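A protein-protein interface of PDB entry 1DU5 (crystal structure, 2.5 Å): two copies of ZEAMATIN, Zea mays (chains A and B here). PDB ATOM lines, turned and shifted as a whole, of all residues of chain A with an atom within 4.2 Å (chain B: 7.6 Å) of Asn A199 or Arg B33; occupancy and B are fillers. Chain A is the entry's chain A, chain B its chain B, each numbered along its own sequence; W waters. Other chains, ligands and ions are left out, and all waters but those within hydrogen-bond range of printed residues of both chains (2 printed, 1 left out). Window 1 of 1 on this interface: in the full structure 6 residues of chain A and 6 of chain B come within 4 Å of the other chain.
Water W2 lies within hydrogen-bond range of the backbone carbonyl oxygen of Asp B113 (3.0 Å) and the guanidinium group of Arg A33 (3.1 Å).
Water W1 bridges OD1 of Asp B113 (3.1 Å) and NH1 of Arg A33 (3.3 Å).
Printed residues of chain B within 4 Å of Asp A113: Arg B33 (2.7 Å).
Of chain B, only Arg B33 comes within 4 Å of Asn A199.
Of the printed residues of chain A, Val B2 touches Arg A33.
Of chain A, only Asp A113 and Asn A199 come within 4 Å of Arg B33.
The nearest residue of chain B that does not touch Asn A199 is Trp B32 (5.3 Å).
The nearest residue of chain A that does not touch Arg B33 is Val A2 (4.1 Å).
The nearest printed residue of chain B that does not touch Val A2 is Arg B33 (4.1 Å).
The guanidinium group (NH1) of Arg B33 is in salt-bridge range of the side-chain carboxylate (OD1) of Asp A113, at 3.8 Å.
The guanidinium group (NH1) of Arg A33 lies within salt-bridge range of the side-chain carboxylate (OD1) of Asp B113 (3.5 Å).
Arg A33 touches Val B2, but with the chains exchanged Val A2 does not touch Arg B33 (4.1 Å).
Arg A33 touches Asp B113, and with the chains exchanged Asp A113 touches Arg B33.
Of the 5 pairs that touch across the chains among the printed residues, 2 have their exchanged pair printed and touching as well.
The backbone NH (N) of Tyr B200 lies within hydrogen-bond range of the backbone carbonyl oxygen (O) of Val B2 (2.8 Å).
N of Val A2 is in hydrogen-bond range of OD1 of Asn A199 (2.8 Å).
The backbone carbonyl oxygen (O) of Val A2 lies within hydrogen-bond range of the backbone NH (N) of Tyr A200 (3.0 Å).
O of Gly A114 lies within hydrogen-bond range of N of Asn A199 (3.0 Å).
NH1 of Arg B33 sits close to OG1 of Thr B4 (3.4 Å).
The backbone carbonyl oxygen (O) of Asn A199 lies within hydrogen-bond range of the backbone NH (N) of Asp A113.
Among the printed residues, merely in contact across the chains: Val A2 with Thr B35, Arg A33 with Val B2 and Asn A199 with Arg B33.
Of the 10 printed residues of chain A, 4 touch a printed residue of chain B.
Hydrophobic or aromatic side chains of chain A that line the printed part of chain B: Val A2.
Hydrophobic or aromatic side chains of chain B that line the printed part of chain A: Val B2.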
ATOM      1  N   ALA A   1      17.811  -4.552 -24.586  1.00  0.00           N
ATOM      2  CA  ALA A   1      16.842  -5.500 -24.108  1.00  0.00           C
ATOM      3  C   ALA A   1      15.749  -4.566 -23.626  1.00  0.00           C
ATOM      4  O   ALA A   1      16.021  -3.373 -23.405  1.00  0.00           O
ATOM      5  CB  ALA A   1      17.360  -6.274 -22.908  1.00  0.00           C
ATOM      6  N   VAL A   2      14.545  -5.088 -23.527  1.00  0.00           N
ATOM      7  CA  VAL A   2      13.421  -4.379 -22.977  1.00  0.00           C
ATOM      8  C   VAL A   2      13.249  -5.064 -21.625  1.00  0.00           C
ATOM      9  O   VAL A   2      13.394  -6.287 -21.485  1.00  0.00           O
ATOM     10  CB  VAL A   2      12.110  -4.564 -23.800  1.00  0.00           C
ATOM     11  CG1 VAL A   2      10.971  -3.870 -23.083  1.00  0.00           C
ATOM     12  CG2 VAL A   2      12.238  -3.960 -25.183  1.00  0.00           C
ATOM     13  N   ARG A  33       7.710  -0.410 -19.383  1.00  0.00           N
ATOM     14  CA  ARG A  33       8.632  -1.136 -20.254  1.00  0.00           C
ATOM     15  C   ARG A  33       9.749  -0.192 -20.669  1.00  0.00           C
ATOM     16  O   ARG A  33       9.503   0.868 -21.244  1.00  0.00           O
ATOM     17  CB  ARG A  33       7.861  -1.684 -21.472  1.00  0.00           C
ATOM     18  CG  ARG A  33       6.986  -2.869 -21.014  1.00  0.00           C
ATOM     19  CD  ARG A  33       6.160  -3.502 -22.119  1.00  0.00           C
ATOM     20  NE  ARG A  33       6.096  -4.953 -21.979  1.00  0.00           N
ATOM     21  CZ  ARG A  33       4.995  -5.618 -21.587  1.00  0.00           C
ATOM     22  NH1 ARG A  33       5.054  -6.943 -21.512  1.00  0.00           N
ATOM     23  NH2 ARG A  33       3.876  -4.999 -21.190  1.00  0.00           N
ATOM     24  N   PRO A 112      14.329 -14.026 -17.438  1.00  0.00           N
ATOM     25  CA  PRO A 112      14.253 -13.939 -18.892  1.00  0.00           C
ATOM     26  C   PRO A 112      12.812 -13.924 -19.382  1.00  0.00           C
ATOM     27  O   PRO A 112      11.944 -14.583 -18.805  1.00  0.00           O
ATOM     28  CB  PRO A 112      15.041 -15.133 -19.364  1.00  0.00           C
ATOM     29  CG  PRO A 112      15.087 -16.041 -18.170  1.00  0.00           C
ATOM     30  CD  PRO A 112      15.269 -15.062 -17.043  1.00  0.00           C
ATOM     31  N   ASP A 113      12.538 -13.184 -20.444  1.00  0.00           N
ATOM     32  CA  ASP A 113      11.178 -13.007 -20.888  1.00  0.00           C
ATOM     33  C   ASP A 113      11.222 -13.122 -22.402  1.00  0.00           C
ATOM     34  O   ASP A 113      10.709 -12.282 -23.137  1.00  0.00           O
ATOM     35  CB  ASP A 113      10.747 -11.627 -20.364  1.00  0.00           C
ATOM     36  CG  ASP A 113       9.270 -11.252 -20.387  1.00  0.00           C
ATOM     37  OD1 ASP A 113       8.977 -10.062 -20.266  1.00  0.00           O
ATOM     38  OD2 ASP A 113       8.404 -12.122 -20.516  1.00  0.00           O
ATOM     39  N   GLY A 114      11.859 -14.179 -22.899  1.00  0.00           N
ATOM     40  CA  GLY A 114      11.933 -14.407 -24.325  1.00  0.00           C
ATOM     41  C   GLY A 114      13.118 -13.677 -24.928  1.00  0.00           C
ATOM     42  O   GLY A 114      13.929 -13.042 -24.244  1.00  0.00           O
ATOM     43  N   GLY A 197      20.165 -10.388 -26.308  1.00  0.00           N
ATOM     44  CA  GLY A 197      18.971 -10.492 -27.152  1.00  0.00           C
ATOM     45  C   GLY A 197      17.753 -10.882 -26.312  1.00  0.00           C
ATOM     46  O   GLY A 197      16.598 -10.670 -26.693  1.00  0.00           O
ATOM     47  N   THR A 198      18.028 -11.494 -25.153  1.00  0.00           N
ATOM     48  CA  THR A 198      17.013 -11.804 -24.159  1.00  0.00           C
ATOM     49  C   THR A 198      16.408 -10.497 -23.663  1.00  0.00           C
ATOM     50  O   THR A 198      17.081  -9.461 -23.654  1.00  0.00           O
ATOM     51  CB  THR A 198      17.652 -12.531 -22.962  1.00  0.00           C
ATOM     52  OG1 THR A 198      18.404 -13.616 -23.515  1.00  0.00           O
ATOM     53  CG2 THR A 198      16.633 -13.102 -21.998  1.00  0.00           C
ATOM     54  N   ASN A 199      15.146 -10.531 -23.249  1.00  0.00           N
ATOM     55  CA  ASN A 199      14.449  -9.397 -22.651  1.00  0.00           C
ATOM     56  C   ASN A 199      14.104  -9.853 -21.241  1.00  0.00           C
ATOM     57  O   ASN A 199      14.184 -11.065 -20.990  1.00  0.00           O
ATOM     58  CB  ASN A 199      13.186  -9.067 -23.443  1.00  0.00           C
ATOM     59  CG  ASN A 199      13.523  -8.516 -24.816  1.00  0.00           C
ATOM     60  OD1 ASN A 199      14.060  -7.423 -24.973  1.00  0.00           O
ATOM     61  ND2 ASN A 199      13.266  -9.218 -25.892  1.00  0.00           N
ATOM     62  N   TYR A 200      13.739  -9.016 -20.261  1.00  0.00           N
ATOM     63  CA  TYR A 200      13.565  -9.504 -18.898  1.00  0.00           C
ATOM     64  C   TYR A 200      12.351  -8.941 -18.212  1.00  0.00           C
ATOM     65  O   TYR A 200      11.783  -7.916 -18.596  1.00  0.00           O
ATOM     66  CB  TYR A 200      14.777  -9.168 -18.036  1.00  0.00           C
ATOM     67  CG  TYR A 200      16.088  -9.738 -18.579  1.00  0.00           C
ATOM     68  CD1 TYR A 200      16.848  -9.023 -19.508  1.00  0.00           C
ATOM     69  CD2 TYR A 200      16.514 -10.994 -18.140  1.00  0.00           C
ATOM     70  CE1 TYR A 200      18.013  -9.558 -20.001  1.00  0.00           C
ATOM     71  CE2 TYR A 200      17.694 -11.539 -18.640  1.00  0.00           C
ATOM     72  CZ  TYR A 200      18.427 -10.808 -19.566  1.00  0.00           C
ATOM     73  OH  TYR A 200      19.594 -11.328 -20.065  1.00  0.00           O
ATOM     74  N   VAL B   2       6.078  -0.321 -26.740  1.00  0.00           N
ATOM     75  CA  VAL B   2       6.795  -1.552 -26.998  1.00  0.00           C
ATOM     76  C   VAL B   2       5.781  -2.521 -27.601  1.00  0.00           C
ATOM     77  O   VAL B   2       4.646  -2.659 -27.126  1.00  0.00           O
ATOM     78  CB  VAL B   2       7.386  -2.119 -25.688  1.00  0.00           C
ATOM     79  CG1 VAL B   2       7.953  -3.529 -25.868  1.00  0.00           C
ATOM     80  CG2 VAL B   2       8.518  -1.208 -25.271  1.00  0.00           C
ATOM     81  N   PHE B   3       6.185  -3.126 -28.716  1.00  0.00           N
ATOM     82  CA  PHE B   3       5.412  -4.136 -29.422  1.00  0.00           C
ATOM     83  C   PHE B   3       6.012  -5.507 -29.179  1.00  0.00           C
ATOM     84  O   PHE B   3       7.181  -5.713 -29.519  1.00  0.00           O
ATOM     85  CB  PHE B   3       5.412  -3.829 -30.933  1.00  0.00           C
ATOM     86  CG  PHE B   3       4.518  -2.629 -31.212  1.00  0.00           C
ATOM     87  CD1 PHE B   3       5.057  -1.343 -31.159  1.00  0.00           C
ATOM     88  CD2 PHE B   3       3.148  -2.814 -31.453  1.00  0.00           C
ATOM     89  CE1 PHE B   3       4.225  -0.242 -31.344  1.00  0.00           C
ATOM     90  CE2 PHE B   3       2.325  -1.701 -31.614  1.00  0.00           C
ATOM     91  CZ  PHE B   3       2.861  -0.415 -31.562  1.00  0.00           C
ATOM     92  N   THR B   4       5.317  -6.434 -28.525  1.00  0.00           N
ATOM     93  CA  THR B   4       5.808  -7.792 -28.414  1.00  0.00           C
ATOM     94  C   THR B   4       4.983  -8.620 -29.396  1.00  0.00           C
ATOM     95  O   THR B   4       3.745  -8.607 -29.442  1.00  0.00           O
ATOM     96  CB  THR B   4       5.681  -8.252 -26.921  1.00  0.00           C
ATOM     97  OG1 THR B   4       6.217  -9.571 -26.815  1.00  0.00           O
ATOM     98  CG2 THR B   4       4.263  -8.266 -26.425  1.00  0.00           C
ATOM     99  N   VAL B   5       5.753  -9.211 -30.300  1.00  0.00           N
ATOM    100  CA  VAL B   5       5.285 -10.062 -31.368  1.00  0.00           C
ATOM    101  C   VAL B   5       5.560 -11.481 -30.884  1.00  0.00           C
ATOM    102  O   VAL B   5       6.733 -11.836 -30.690  1.00  0.00           O
ATOM    103  CB  VAL B   5       6.089  -9.751 -32.659  1.00  0.00           C
ATOM    104  CG1 VAL B   5       5.590 -10.606 -33.785  1.00  0.00           C
ATOM    105  CG2 VAL B   5       5.925  -8.303 -33.070  1.00  0.00           C
ATOM    106  N   VAL B   6       4.539 -12.295 -30.655  1.00  0.00           N
ATOM    107  CA  VAL B   6       4.757 -13.674 -30.238  1.00  0.00           C
ATOM    108  C   VAL B   6       4.285 -14.560 -31.389  1.00  0.00           C
ATOM    109  O   VAL B   6       3.191 -14.347 -31.939  1.00  0.00           O
ATOM    110  CB  VAL B   6       3.942 -14.016 -28.952  1.00  0.00           C
ATOM    111  CG1 VAL B   6       4.367 -15.392 -28.465  1.00  0.00           C
ATOM    112  CG2 VAL B   6       4.165 -12.992 -27.852  1.00  0.00           C
ATOM    113  N   GLY B  21      12.340  -2.215 -36.744  1.00  0.00           N
ATOM    114  CA  GLY B  21      12.476  -3.663 -36.639  1.00  0.00           C
ATOM    115  C   GLY B  21      12.959  -4.282 -37.942  1.00  0.00           C
ATOM    116  O   GLY B  21      14.094  -4.758 -38.046  1.00  0.00           O
ATOM    117  N   ARG B  24      12.469 -10.651 -38.750  1.00  0.00           N
ATOM    118  CA  ARG B  24      13.119 -11.638 -37.910  1.00  0.00           C
ATOM    119  C   ARG B  24      12.303 -12.920 -37.911  1.00  0.00           C
ATOM    120  O   ARG B  24      11.066 -12.906 -37.873  1.00  0.00           O
ATOM    121  CB  ARG B  24      13.243 -11.092 -36.487  1.00  0.00           C
ATOM    122  CG  ARG B  24      13.955 -11.981 -35.489  1.00  0.00           C
ATOM    123  CD  ARG B  24      14.219 -11.186 -34.229  1.00  0.00           C
ATOM    124  NE  ARG B  24      15.299 -10.214 -34.402  1.00  0.00           N
ATOM    125  CZ  ARG B  24      15.666  -9.390 -33.420  1.00  0.00           C
ATOM    126  NH1 ARG B  24      16.658  -8.526 -33.617  1.00  0.00           N
ATOM    127  NH2 ARG B  24      15.046  -9.392 -32.250  1.00  0.00           N
ATOM    128  N   LEU B  26      10.896 -16.244 -36.421  1.00  0.00           N
ATOM    129  CA  LEU B  26      10.379 -16.662 -35.136  1.00  0.00           C
ATOM    130  C   LEU B  26       9.863 -18.081 -35.280  1.00  0.00           C
ATOM    131  O   LEU B  26       9.057 -18.400 -36.162  1.00  0.00           O
ATOM    132  CB  LEU B  26       9.213 -15.789 -34.664  1.00  0.00           C
ATOM    133  CG  LEU B  26       9.394 -14.303 -34.382  1.00  0.00           C
ATOM    134  CD1 LEU B  26       8.051 -13.746 -33.944  1.00  0.00           C
ATOM    135  CD2 LEU B  26      10.448 -14.068 -33.301  1.00  0.00           C
ATOM    136  N   SER B  31       9.309 -14.908 -29.194  1.00  0.00           N
ATOM    137  CA  SER B  31       8.835 -13.548 -29.091  1.00  0.00           C
ATOM    138  C   SER B  31       9.914 -12.577 -29.562  1.00  0.00           C
ATOM    139  O   SER B  31      11.122 -12.854 -29.518  1.00  0.00           O
ATOM    140  CB  SER B  31       8.453 -13.253 -27.640  1.00  0.00           C
ATOM    141  OG  SER B  31       7.282 -13.960 -27.254  1.00  0.00           O
ATOM    142  N   TRP B  32       9.459 -11.412 -29.996  1.00  0.00           N
ATOM    143  CA  TRP B  32      10.294 -10.355 -30.503  1.00  0.00           C
ATOM    144  C   TRP B  32       9.738  -9.116 -29.826  1.00  0.00           C
ATOM    145  O   TRP B  32       8.521  -9.023 -29.648  1.00  0.00           O
ATOM    146  CB  TRP B  32      10.122 -10.276 -32.010  1.00  0.00           C
ATOM    147  CG  TRP B  32      11.009  -9.276 -32.743  1.00  0.00           C
ATOM    148  CD1 TRP B  32      12.138  -8.739 -32.185  1.00  0.00           C
ATOM    149  CD2 TRP B  32      10.799  -8.840 -34.021  1.00  0.00           C
ATOM    150  NE1 TRP B  32      12.651  -7.977 -33.108  1.00  0.00           N
ATOM    151  CE2 TRP B  32      11.901  -8.001 -34.219  1.00  0.00           C
ATOM    152  CE3 TRP B  32       9.865  -9.037 -35.035  1.00  0.00           C
ATOM    153  CZ2 TRP B  32      12.069  -7.353 -35.438  1.00  0.00           C
ATOM    154  CZ3 TRP B  32      10.041  -8.378 -36.253  1.00  0.00           C
ATOM    155  CH2 TRP B  32      11.139  -7.543 -36.454  1.00  0.00           C
ATOM    156  N   ARG B  33      10.556  -8.167 -29.386  1.00  0.00           N
ATOM    157  CA  ARG B  33      10.077  -6.959 -28.740  1.00  0.00           C
ATOM    158  C   ARG B  33      10.743  -5.812 -29.462  1.00  0.00           C
ATOM    159  O   ARG B  33      11.951  -5.769 -29.681  1.00  0.00           O
ATOM    160  CB  ARG B  33      10.442  -6.953 -27.256  1.00  0.00           C
ATOM    161  CG  ARG B  33       9.395  -7.767 -26.522  1.00  0.00           C
ATOM    162  CD  ARG B  33       9.544  -7.699 -25.014  1.00  0.00           C
ATOM    163  NE  ARG B  33       8.333  -8.219 -24.404  1.00  0.00           N
ATOM    164  CZ  ARG B  33       8.220  -9.502 -24.050  1.00  0.00           C
ATOM    165  NH1 ARG B  33       7.088  -9.930 -23.514  1.00  0.00           N
ATOM    166  NH2 ARG B  33       9.214 -10.366 -24.200  1.00  0.00           N
ATOM    167  N   ILE B  34       9.864  -4.922 -29.882  1.00  0.00           N
ATOM    168  CA  ILE B  34      10.189  -3.796 -30.738  1.00  0.00           C
ATOM    169  C   ILE B  34       9.819  -2.553 -29.940  1.00  0.00           C
ATOM    170  O   ILE B  34       8.905  -2.582 -29.105  1.00  0.00           O
ATOM    171  CB  ILE B  34       9.345  -3.942 -32.041  1.00  0.00           C
ATOM    172  CG1 ILE B  34       9.739  -5.202 -32.797  1.00  0.00           C
ATOM    173  CG2 ILE B  34       9.550  -2.739 -32.943  1.00  0.00           C
ATOM    174  CD1 ILE B  34       8.718  -5.615 -33.882  1.00  0.00           C
ATOM    175  N   THR B  35      10.510  -1.440 -30.120  1.00  0.00           N
ATOM    176  CA  THR B  35      10.170  -0.219 -29.436  1.00  0.00           C
ATOM    177  C   THR B  35       9.928   0.782 -30.549  1.00  0.00           C
ATOM    178  O   THR B  35      10.810   1.061 -31.361  1.00  0.00           O
ATOM    179  CB  THR B  35      11.349   0.177 -28.502  1.00  0.00           C
ATOM    180  OG1 THR B  35      11.511  -0.909 -27.585  1.00  0.00           O
ATOM    181  CG2 THR B  35      11.116   1.464 -27.722  1.00  0.00           C
ATOM    182  N   ALA B  36       8.696   1.255 -30.674  1.00  0.00           N
ATOM    183  CA  ALA B  36       8.367   2.270 -31.661  1.00  0.00           C
ATOM    184  C   ALA B  36       8.264   3.628 -30.974  1.00  0.00           C
ATOM    185  O   ALA B  36       7.624   3.747 -29.909  1.00  0.00           O
ATOM    186  CB  ALA B  36       7.035   1.953 -32.322  1.00  0.00           C
ATOM    187  N   ASP B 113      -1.218  -3.962 -23.963  1.00  0.00           N
ATOM    188  CA  ASP B 113      -0.407  -4.776 -23.092  1.00  0.00           C
ATOM    189  C   ASP B 113       0.192  -3.907 -21.999  1.00  0.00           C
ATOM    190  O   ASP B 113       1.395  -3.937 -21.709  1.00  0.00           O
ATOM    191  CB  ASP B 113       0.664  -5.438 -23.955  1.00  0.00           C
ATOM    192  CG  ASP B 113       1.236  -6.759 -23.459  1.00  0.00           C
ATOM    193  OD1 ASP B 113       2.379  -7.059 -23.813  1.00  0.00           O
ATOM    194  OD2 ASP B 113       0.541  -7.508 -22.762  1.00  0.00           O
ATOM    195  N   TYR B 200       1.883  -2.858 -26.690  1.00  0.00           N
ATOM    196  CA  TYR B 200       0.971  -3.712 -27.421  1.00  0.00           C
ATOM    197  C   TYR B 200       1.516  -5.099 -27.639  1.00  0.00           C
ATOM    198  O   TYR B 200       2.726  -5.353 -27.589  1.00  0.00           O
ATOM    199  CB  TYR B 200       0.660  -3.091 -28.775  1.00  0.00           C
ATOM    200  CG  TYR B 200      -0.071  -1.769 -28.690  1.00  0.00           C
ATOM    201  CD1 TYR B 200       0.637  -0.568 -28.757  1.00  0.00           C
ATOM    202  CD2 TYR B 200      -1.466  -1.769 -28.577  1.00  0.00           C
ATOM    203  CE1 TYR B 200      -0.032   0.638 -28.726  1.00  0.00           C
ATOM    204  CE2 TYR B 200      -2.158  -0.560 -28.535  1.00  0.00           C
ATOM    205  CZ  TYR B 200      -1.427   0.628 -28.613  1.00  0.00           C
ATOM    206  OH  TYR B 200      -2.092   1.823 -28.578  1.00  0.00           O
ATOM    207  N   LYS B 201       0.578  -5.997 -27.894  1.00  0.00           N
ATOM    208  CA  LYS B 201       0.869  -7.392 -28.112  1.00  0.00           C
ATOM    209  C   LYS B 201       0.211  -7.823 -29.404  1.00  0.00           C
ATOM    210  O   LYS B 201      -0.983  -7.582 -29.611  1.00  0.00           O
ATOM    211  CB  LYS B 201       0.344  -8.169 -26.907  1.00  0.00           C
ATOM    212  CG  LYS B 201       0.863  -9.580 -26.880  1.00  0.00           C
ATOM    213  CD  LYS B 201       0.689 -10.268 -25.538  1.00  0.00           C
ATOM    214  CE  LYS B 201       1.534 -11.525 -25.641  1.00  0.00           C
ATOM    215  NZ  LYS B 201       1.710 -12.164 -24.351  1.00  0.00           N
HETATM  216  O   HOH W   1       3.277  -9.627 -22.328  1.00  0.00           O
HETATM  217  O   HOH W   2       3.210  -2.262 -19.961  1.00  0.00           O
